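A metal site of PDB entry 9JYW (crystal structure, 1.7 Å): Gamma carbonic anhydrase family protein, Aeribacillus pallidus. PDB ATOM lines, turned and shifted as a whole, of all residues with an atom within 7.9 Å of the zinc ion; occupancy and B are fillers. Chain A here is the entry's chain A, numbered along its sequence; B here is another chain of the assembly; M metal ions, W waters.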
ATOM      1  N   ARG A  45      12.192 -33.722  13.203  1.00  0.00           N
ATOM      2  CA  ARG A  45      12.118 -33.910  14.664  1.00  0.00           C
ATOM      3  C   ARG A  45      10.968 -34.844  14.972  1.00  0.00           C
ATOM      4  O   ARG A  45       9.829 -34.452  14.752  1.00  0.00           O
ATOM      5  CB  ARG A  45      11.945 -32.587  15.422  1.00  0.00           C
ATOM      6  CG  ARG A  45      13.254 -31.847  15.645  1.00  0.00           C
ATOM      7  CD  ARG A  45      13.145 -30.872  16.779  1.00  0.00           C
ATOM      8  NE  ARG A  45      12.291 -29.750  16.472  1.00  0.00           N
ATOM      9  CZ  ARG A  45      11.224 -29.364  17.149  1.00  0.00           C
ATOM     10  NH1 ARG A  45      10.731 -30.091  18.142  1.00  0.00           N
ATOM     11  NH2 ARG A  45      10.568 -28.283  16.747  1.00  0.00           N
ATOM     12  N   ASP A  47       9.478 -35.947  17.766  1.00  0.00           N
ATOM     13  CA  ASP A  47       9.325 -35.815  19.235  1.00  0.00           C
ATOM     14  C   ASP A  47       7.872 -35.525  19.643  1.00  0.00           C
ATOM     15  O   ASP A  47       7.646 -35.270  20.849  1.00  0.00           O
ATOM     16  CB  ASP A  47      10.281 -34.761  19.798  1.00  0.00           C
ATOM     17  CG  ASP A  47      10.255 -33.408  19.082  1.00  0.00           C
ATOM     18  OD1 ASP A  47       9.190 -33.047  18.520  1.00  0.00           O
ATOM     19  OD2 ASP A  47      11.305 -32.716  19.140  1.00  0.00           O
ATOM     20  N   VAL A  48       6.917 -35.544  18.708  1.00  0.00           N
ATOM     21  CA  VAL A  48       5.486 -35.296  19.034  1.00  0.00           C
ATOM     22  C   VAL A  48       4.652 -36.520  18.617  1.00  0.00           C
ATOM     23  O   VAL A  48       3.797 -36.952  19.413  1.00  0.00           O
ATOM     24  CB  VAL A  48       4.972 -33.977  18.411  1.00  0.00           C
ATOM     25  CG1 VAL A  48       3.477 -33.828  18.604  1.00  0.00           C
ATOM     26  CG2 VAL A  48       5.706 -32.805  18.990  1.00  0.00           C
ATOM     27  N   CYS A  64      11.415 -28.969   6.601  1.00  0.00           N
ATOM     28  CA  CYS A  64      11.104 -29.110   8.034  1.00  0.00           C
ATOM     29  C   CYS A  64       9.944 -30.093   8.170  1.00  0.00           C
ATOM     30  O   CYS A  64       8.927 -29.844   7.585  1.00  0.00           O
ATOM     31  CB  CYS A  64      10.753 -27.782   8.657  1.00  0.00           C
ATOM     32  SG  CYS A  64      10.444 -27.926  10.432  1.00  0.00           S
ATOM     33  N   LEU A  65      10.177 -31.203   8.844  1.00  0.00           N
ATOM     34  CA  LEU A  65       9.176 -32.283   9.062  1.00  0.00           C
ATOM     35  C   LEU A  65       8.903 -32.338  10.563  1.00  0.00           C
ATOM     36  O   LEU A  65       9.863 -32.528  11.344  1.00  0.00           O
ATOM     37  CB  LEU A  65       9.761 -33.595   8.540  1.00  0.00           C
ATOM     38  CG  LEU A  65       9.524 -33.882   7.060  1.00  0.00           C
ATOM     39  CD1 LEU A  65      10.135 -32.826   6.158  1.00  0.00           C
ATOM     40  CD2 LEU A  65      10.045 -35.248   6.677  1.00  0.00           C
ATOM     41  N   HIS A  66       7.651 -32.138  10.947  1.00  0.00           N
ATOM     42  CA  HIS A  66       7.261 -32.132  12.381  1.00  0.00           C
ATOM     43  C   HIS A  66       5.840 -32.671  12.497  1.00  0.00           C
ATOM     44  O   HIS A  66       5.245 -33.055  11.458  1.00  0.00           O
ATOM     45  CB  HIS A  66       7.461 -30.753  13.048  1.00  0.00           C
ATOM     46  CG  HIS A  66       7.619 -30.878  14.541  1.00  0.00           C
ATOM     47  ND1 HIS A  66       7.023 -30.079  15.396  1.00  0.00           N
ATOM     48  CD2 HIS A  66       8.289 -31.754  15.309  1.00  0.00           C
ATOM     49  CE1 HIS A  66       7.223 -30.357  16.621  1.00  0.00           C
ATOM     50  NE2 HIS A  66       8.030 -31.421  16.630  1.00  0.00           N
ATOM     51  N   GLN A  67       5.350 -32.796  13.742  1.00  0.00           N
ATOM     52  CA  GLN A  67       3.989 -33.334  13.963  1.00  0.00           C
ATOM     53  C   GLN A  67       3.275 -32.501  15.025  1.00  0.00           C
ATOM     54  O   GLN A  67       3.965 -31.887  15.874  1.00  0.00           O
ATOM     55  CB  GLN A  67       4.015 -34.789  14.436  1.00  0.00           C
ATOM     56  CG  GLN A  67       5.091 -35.658  13.781  1.00  0.00           C
ATOM     57  CD  GLN A  67       6.437 -35.456  14.414  1.00  0.00           C
ATOM     58  OE1 GLN A  67       6.586 -35.271  15.631  1.00  0.00           O
ATOM     59  NE2 GLN A  67       7.454 -35.475  13.578  1.00  0.00           N
ATOM     60  N   SER A  68       1.949 -32.603  15.034  1.00  0.00           N
ATOM     61  CA  SER A  68       1.063 -32.206  16.123  1.00  0.00           C
ATOM     62  C   SER A  68       0.615 -33.473  16.845  1.00  0.00           C
ATOM     63  O   SER A  68       0.745 -34.577  16.325  1.00  0.00           O
ATOM     64  CB  SER A  68      -0.101 -31.409  15.599  1.00  0.00           C
ATOM     65  OG  SER A  68       0.334 -30.159  15.146  1.00  0.00           O
ATOM     66  N   LEU A  86       7.583 -27.457   4.131  1.00  0.00           N
ATOM     67  CA  LEU A  86       7.161 -27.724   5.526  1.00  0.00           C
ATOM     68  C   LEU A  86       6.078 -28.793   5.486  1.00  0.00           C
ATOM     69  O   LEU A  86       5.039 -28.533   4.852  1.00  0.00           O
ATOM     70  CB  LEU A  86       6.647 -26.399   6.093  1.00  0.00           C
ATOM     71  CG  LEU A  86       6.180 -26.357   7.536  1.00  0.00           C
ATOM     72  CD1 LEU A  86       7.057 -27.080   8.513  1.00  0.00           C
ATOM     73  CD2 LEU A  86       5.992 -24.899   7.948  1.00  0.00           C
ATOM     74  N   LEU A  87       6.325 -29.930   6.105  1.00  0.00           N
ATOM     75  CA  LEU A  87       5.311 -31.000   6.329  1.00  0.00           C
ATOM     76  C   LEU A  87       5.010 -31.050   7.812  1.00  0.00           C
ATOM     77  O   LEU A  87       5.942 -31.281   8.604  1.00  0.00           O
ATOM     78  CB  LEU A  87       5.845 -32.345   5.821  1.00  0.00           C
ATOM     79  CG  LEU A  87       6.219 -32.419   4.352  1.00  0.00           C
ATOM     80  CD1 LEU A  87       6.745 -33.808   4.005  1.00  0.00           C
ATOM     81  CD2 LEU A  87       5.079 -32.059   3.453  1.00  0.00           C
ATOM     82  N   HIS A  88       3.743 -30.883   8.187  1.00  0.00           N
ATOM     83  CA  HIS A  88       3.349 -30.919   9.617  1.00  0.00           C
ATOM     84  C   HIS A  88       2.226 -31.951   9.748  1.00  0.00           C
ATOM     85  O   HIS A  88       1.118 -31.606   9.356  1.00  0.00           O
ATOM     86  CB  HIS A  88       3.000 -29.524  10.096  1.00  0.00           C
ATOM     87  CG  HIS A  88       3.356 -29.315  11.542  1.00  0.00           C
ATOM     88  ND1 HIS A  88       2.479 -29.663  12.548  1.00  0.00           N
ATOM     89  CD2 HIS A  88       4.476 -28.864  12.191  1.00  0.00           C
ATOM     90  CE1 HIS A  88       3.025 -29.426  13.701  1.00  0.00           C
ATOM     91  NE2 HIS A  88       4.162 -28.934  13.498  1.00  0.00           N
ATOM     92  N   SER A  89       2.531 -33.166  10.185  1.00  0.00           N
ATOM     93  CA  SER A  89       1.499 -34.228  10.341  1.00  0.00           C
ATOM     94  C   SER A  89       0.762 -34.458   9.010  1.00  0.00           C
ATOM     95  O   SER A  89      -0.455 -34.723   9.027  1.00  0.00           O
ATOM     96  CB  SER A  89       0.554 -33.894  11.499  1.00  0.00           C
ATOM     97  OG  SER A  89       1.182 -34.094  12.746  1.00  0.00           O
ATOM     98  N   ASP A 106      -1.587 -29.995   9.132  1.00  0.00           N
ATOM     99  CA  ASP A 106      -2.068 -31.135   9.899  1.00  0.00           C
ATOM    100  C   ASP A 106      -3.217 -31.939   9.338  1.00  0.00           C
ATOM    101  O   ASP A 106      -4.269 -31.436   9.132  1.00  0.00           O
ATOM    102  CB  ASP A 106      -2.402 -30.735  11.349  1.00  0.00           C
ATOM    103  CG  ASP A 106      -1.208 -30.278  12.179  1.00  0.00           C
ATOM    104  OD1 ASP A 106      -0.039 -30.539  11.837  1.00  0.00           O
ATOM    105  OD2 ASP A 106      -1.462 -29.684  13.234  1.00  0.00           O
ATOM    106  N   GLN B  60      11.113 -21.665  16.602  1.00  0.00           N
ATOM    107  CA  GLN B  60      11.184 -23.040  16.068  1.00  0.00           C
ATOM    108  C   GLN B  60      12.228 -23.127  14.937  1.00  0.00           C
ATOM    109  O   GLN B  60      12.990 -22.180  14.707  1.00  0.00           O
ATOM    110  CB  GLN B  60       9.777 -23.522  15.733  1.00  0.00           C
ATOM    111  CG  GLN B  60       8.936 -23.716  16.972  1.00  0.00           C
ATOM    112  CD  GLN B  60       7.509 -24.035  16.649  1.00  0.00           C
ATOM    113  OE1 GLN B  60       7.159 -24.526  15.578  1.00  0.00           O
ATOM    114  NE2 GLN B  60       6.636 -23.716  17.566  1.00  0.00           N
ATOM    115  N   ASP B  61      12.311 -24.299  14.334  1.00  0.00           N
ATOM    116  CA  ASP B  61      13.416 -24.671  13.415  1.00  0.00           C
ATOM    117  C   ASP B  61      13.389 -23.776  12.156  1.00  0.00           C
ATOM    118  O   ASP B  61      12.323 -23.434  11.660  1.00  0.00           O
ATOM    119  CB  ASP B  61      13.310 -26.146  13.042  1.00  0.00           C
ATOM    120  CG  ASP B  61      12.821 -27.009  14.191  1.00  0.00           C
ATOM    121  OD1 ASP B  61      11.616 -26.901  14.548  1.00  0.00           O
ATOM    122  OD2 ASP B  61      13.650 -27.689  14.779  1.00  0.00           O
ATOM    123  N   GLY B  82       6.586 -20.159  14.961  1.00  0.00           N
ATOM    124  CA  GLY B  82       6.493 -21.412  14.207  1.00  0.00           C
ATOM    125  C   GLY B  82       7.669 -21.705  13.302  1.00  0.00           C
ATOM    126  O   GLY B  82       8.462 -20.818  13.004  1.00  0.00           O
ATOM    127  N   HIS B  83       7.777 -22.968  12.873  1.00  0.00           N
ATOM    128  CA  HIS B  83       8.850 -23.405  11.946  1.00  0.00           C
ATOM    129  C   HIS B  83       8.942 -22.471  10.739  1.00  0.00           C
ATOM    130  O   HIS B  83       7.893 -22.124  10.204  1.00  0.00           O
ATOM    131  CB  HIS B  83       8.635 -24.803  11.414  1.00  0.00           C
ATOM    132  CG  HIS B  83       8.201 -25.815  12.431  1.00  0.00           C
ATOM    133  ND1 HIS B  83       9.107 -26.404  13.291  1.00  0.00           N
ATOM    134  CD2 HIS B  83       7.004 -26.353  12.700  1.00  0.00           C
ATOM    135  CE1 HIS B  83       8.441 -27.300  14.023  1.00  0.00           C
ATOM    136  NE2 HIS B  83       7.216 -27.209  13.684  1.00  0.00           N
ATOM    137  N   MET B 100       3.594 -21.229  11.678  1.00  0.00           N
ATOM    138  CA  MET B 100       4.683 -21.773  10.833  1.00  0.00           C
ATOM    139  C   MET B 100       4.557 -21.283   9.385  1.00  0.00           C
ATOM    140  O   MET B 100       3.442 -21.175   8.850  1.00  0.00           O
ATOM    141  CB  MET B 100       4.688 -23.299  10.948  1.00  0.00           C
ATOM    142  CG  MET B 100       3.444 -23.952  10.365  1.00  0.00           C
ATOM    143  SD  MET B 100       3.493 -25.750  10.717  1.00  0.00           S
ATOM    144  CE  MET B 100       2.628 -25.843  12.268  1.00  0.00           C
ATOM    145  N   ILE B 156       1.148 -25.535  23.551  1.00  0.00           N
ATOM    146  CA  ILE B 156       2.345 -25.518  22.667  1.00  0.00           C
ATOM    147  C   ILE B 156       3.525 -24.863  23.412  1.00  0.00           C
ATOM    148  O   ILE B 156       4.618 -25.438  23.411  1.00  0.00           O
ATOM    149  CB  ILE B 156       2.056 -24.798  21.334  1.00  0.00           C
ATOM    150  CG1 ILE B 156       1.044 -25.596  20.503  1.00  0.00           C
ATOM    151  CG2 ILE B 156       3.344 -24.538  20.578  1.00  0.00           C
ATOM    152  CD1 ILE B 156       0.474 -24.842  19.320  1.00  0.00           C
ATOM    153  N   TYR B 160       7.035 -26.845  24.565  1.00  0.00           N
ATOM    154  CA  TYR B 160       8.362 -26.443  24.035  1.00  0.00           C
ATOM    155  C   TYR B 160       9.377 -26.224  25.172  1.00  0.00           C
ATOM    156  O   TYR B 160      10.553 -26.580  25.042  1.00  0.00           O
ATOM    157  CB  TYR B 160       8.225 -25.248  23.101  1.00  0.00           C
ATOM    158  CG  TYR B 160       8.150 -25.678  21.657  1.00  0.00           C
ATOM    159  CD1 TYR B 160       9.314 -25.997  20.971  1.00  0.00           C
ATOM    160  CD2 TYR B 160       6.943 -25.820  21.015  1.00  0.00           C
ATOM    161  CE1 TYR B 160       9.277 -26.444  19.652  1.00  0.00           C
ATOM    162  CE2 TYR B 160       6.884 -26.258  19.701  1.00  0.00           C
ATOM    163  CZ  TYR B 160       8.054 -26.554  19.023  1.00  0.00           C
ATOM    164  OH  TYR B 160       8.012 -27.017  17.737  1.00  0.00           O
HETATM  165 ZN    ZN M   1       5.805 -28.420  14.762  1.00  0.00          ZN
HETATM  166  O   HOH W   1       5.069 -27.341  16.693  1.00  0.00           O
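A ring nitrogen (ND1) of His 88 lies within hydrogen-bond range of the side-chain carboxylate of Asp 106.
The backbone NH of His 83 of chain B sits at hydrogen-bond distance from the side-chain amide oxygen of Gln 60 of chain B.
ND1 of His 83 of chain B is in hydrogen-bond range of OD1 of Asp 61 of chain B (2.8 Å).
A ring nitrogen (ND1) of His 83 of chain B lies within hydrogen-bond range of the side-chain sulfur (SG) of Cys 64.
NE2 of His 66 is in hydrogen-bond range of NH1 of Arg 45 (3.4 Å).
The backbone carbonyl oxygen (O) of Leu 87 is in hydrogen-bond range of the backbone NH (N) of His 66, at 3.0 Å.
The backbone carbonyl oxygen (O) of His 66 lies within hydrogen-bond range of the backbone NH (N) of Ser 89.
The side-chain hydroxyl (OH) of Tyr 160 of chain B is in hydrogen-bond range of the guanidinium group (NH2) of Arg 45 (3.0 Å).
Residues that only touch the zinc ion: Tyr 160 of chain B (3.96 Å).
The zinc ion is bound by NE2 of His 88 (2.1 Å), NE2 of His 83 of chain B (2.1 Å), ND1 of His 66 (2.2 Å) and water W1 (2.3 Å).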
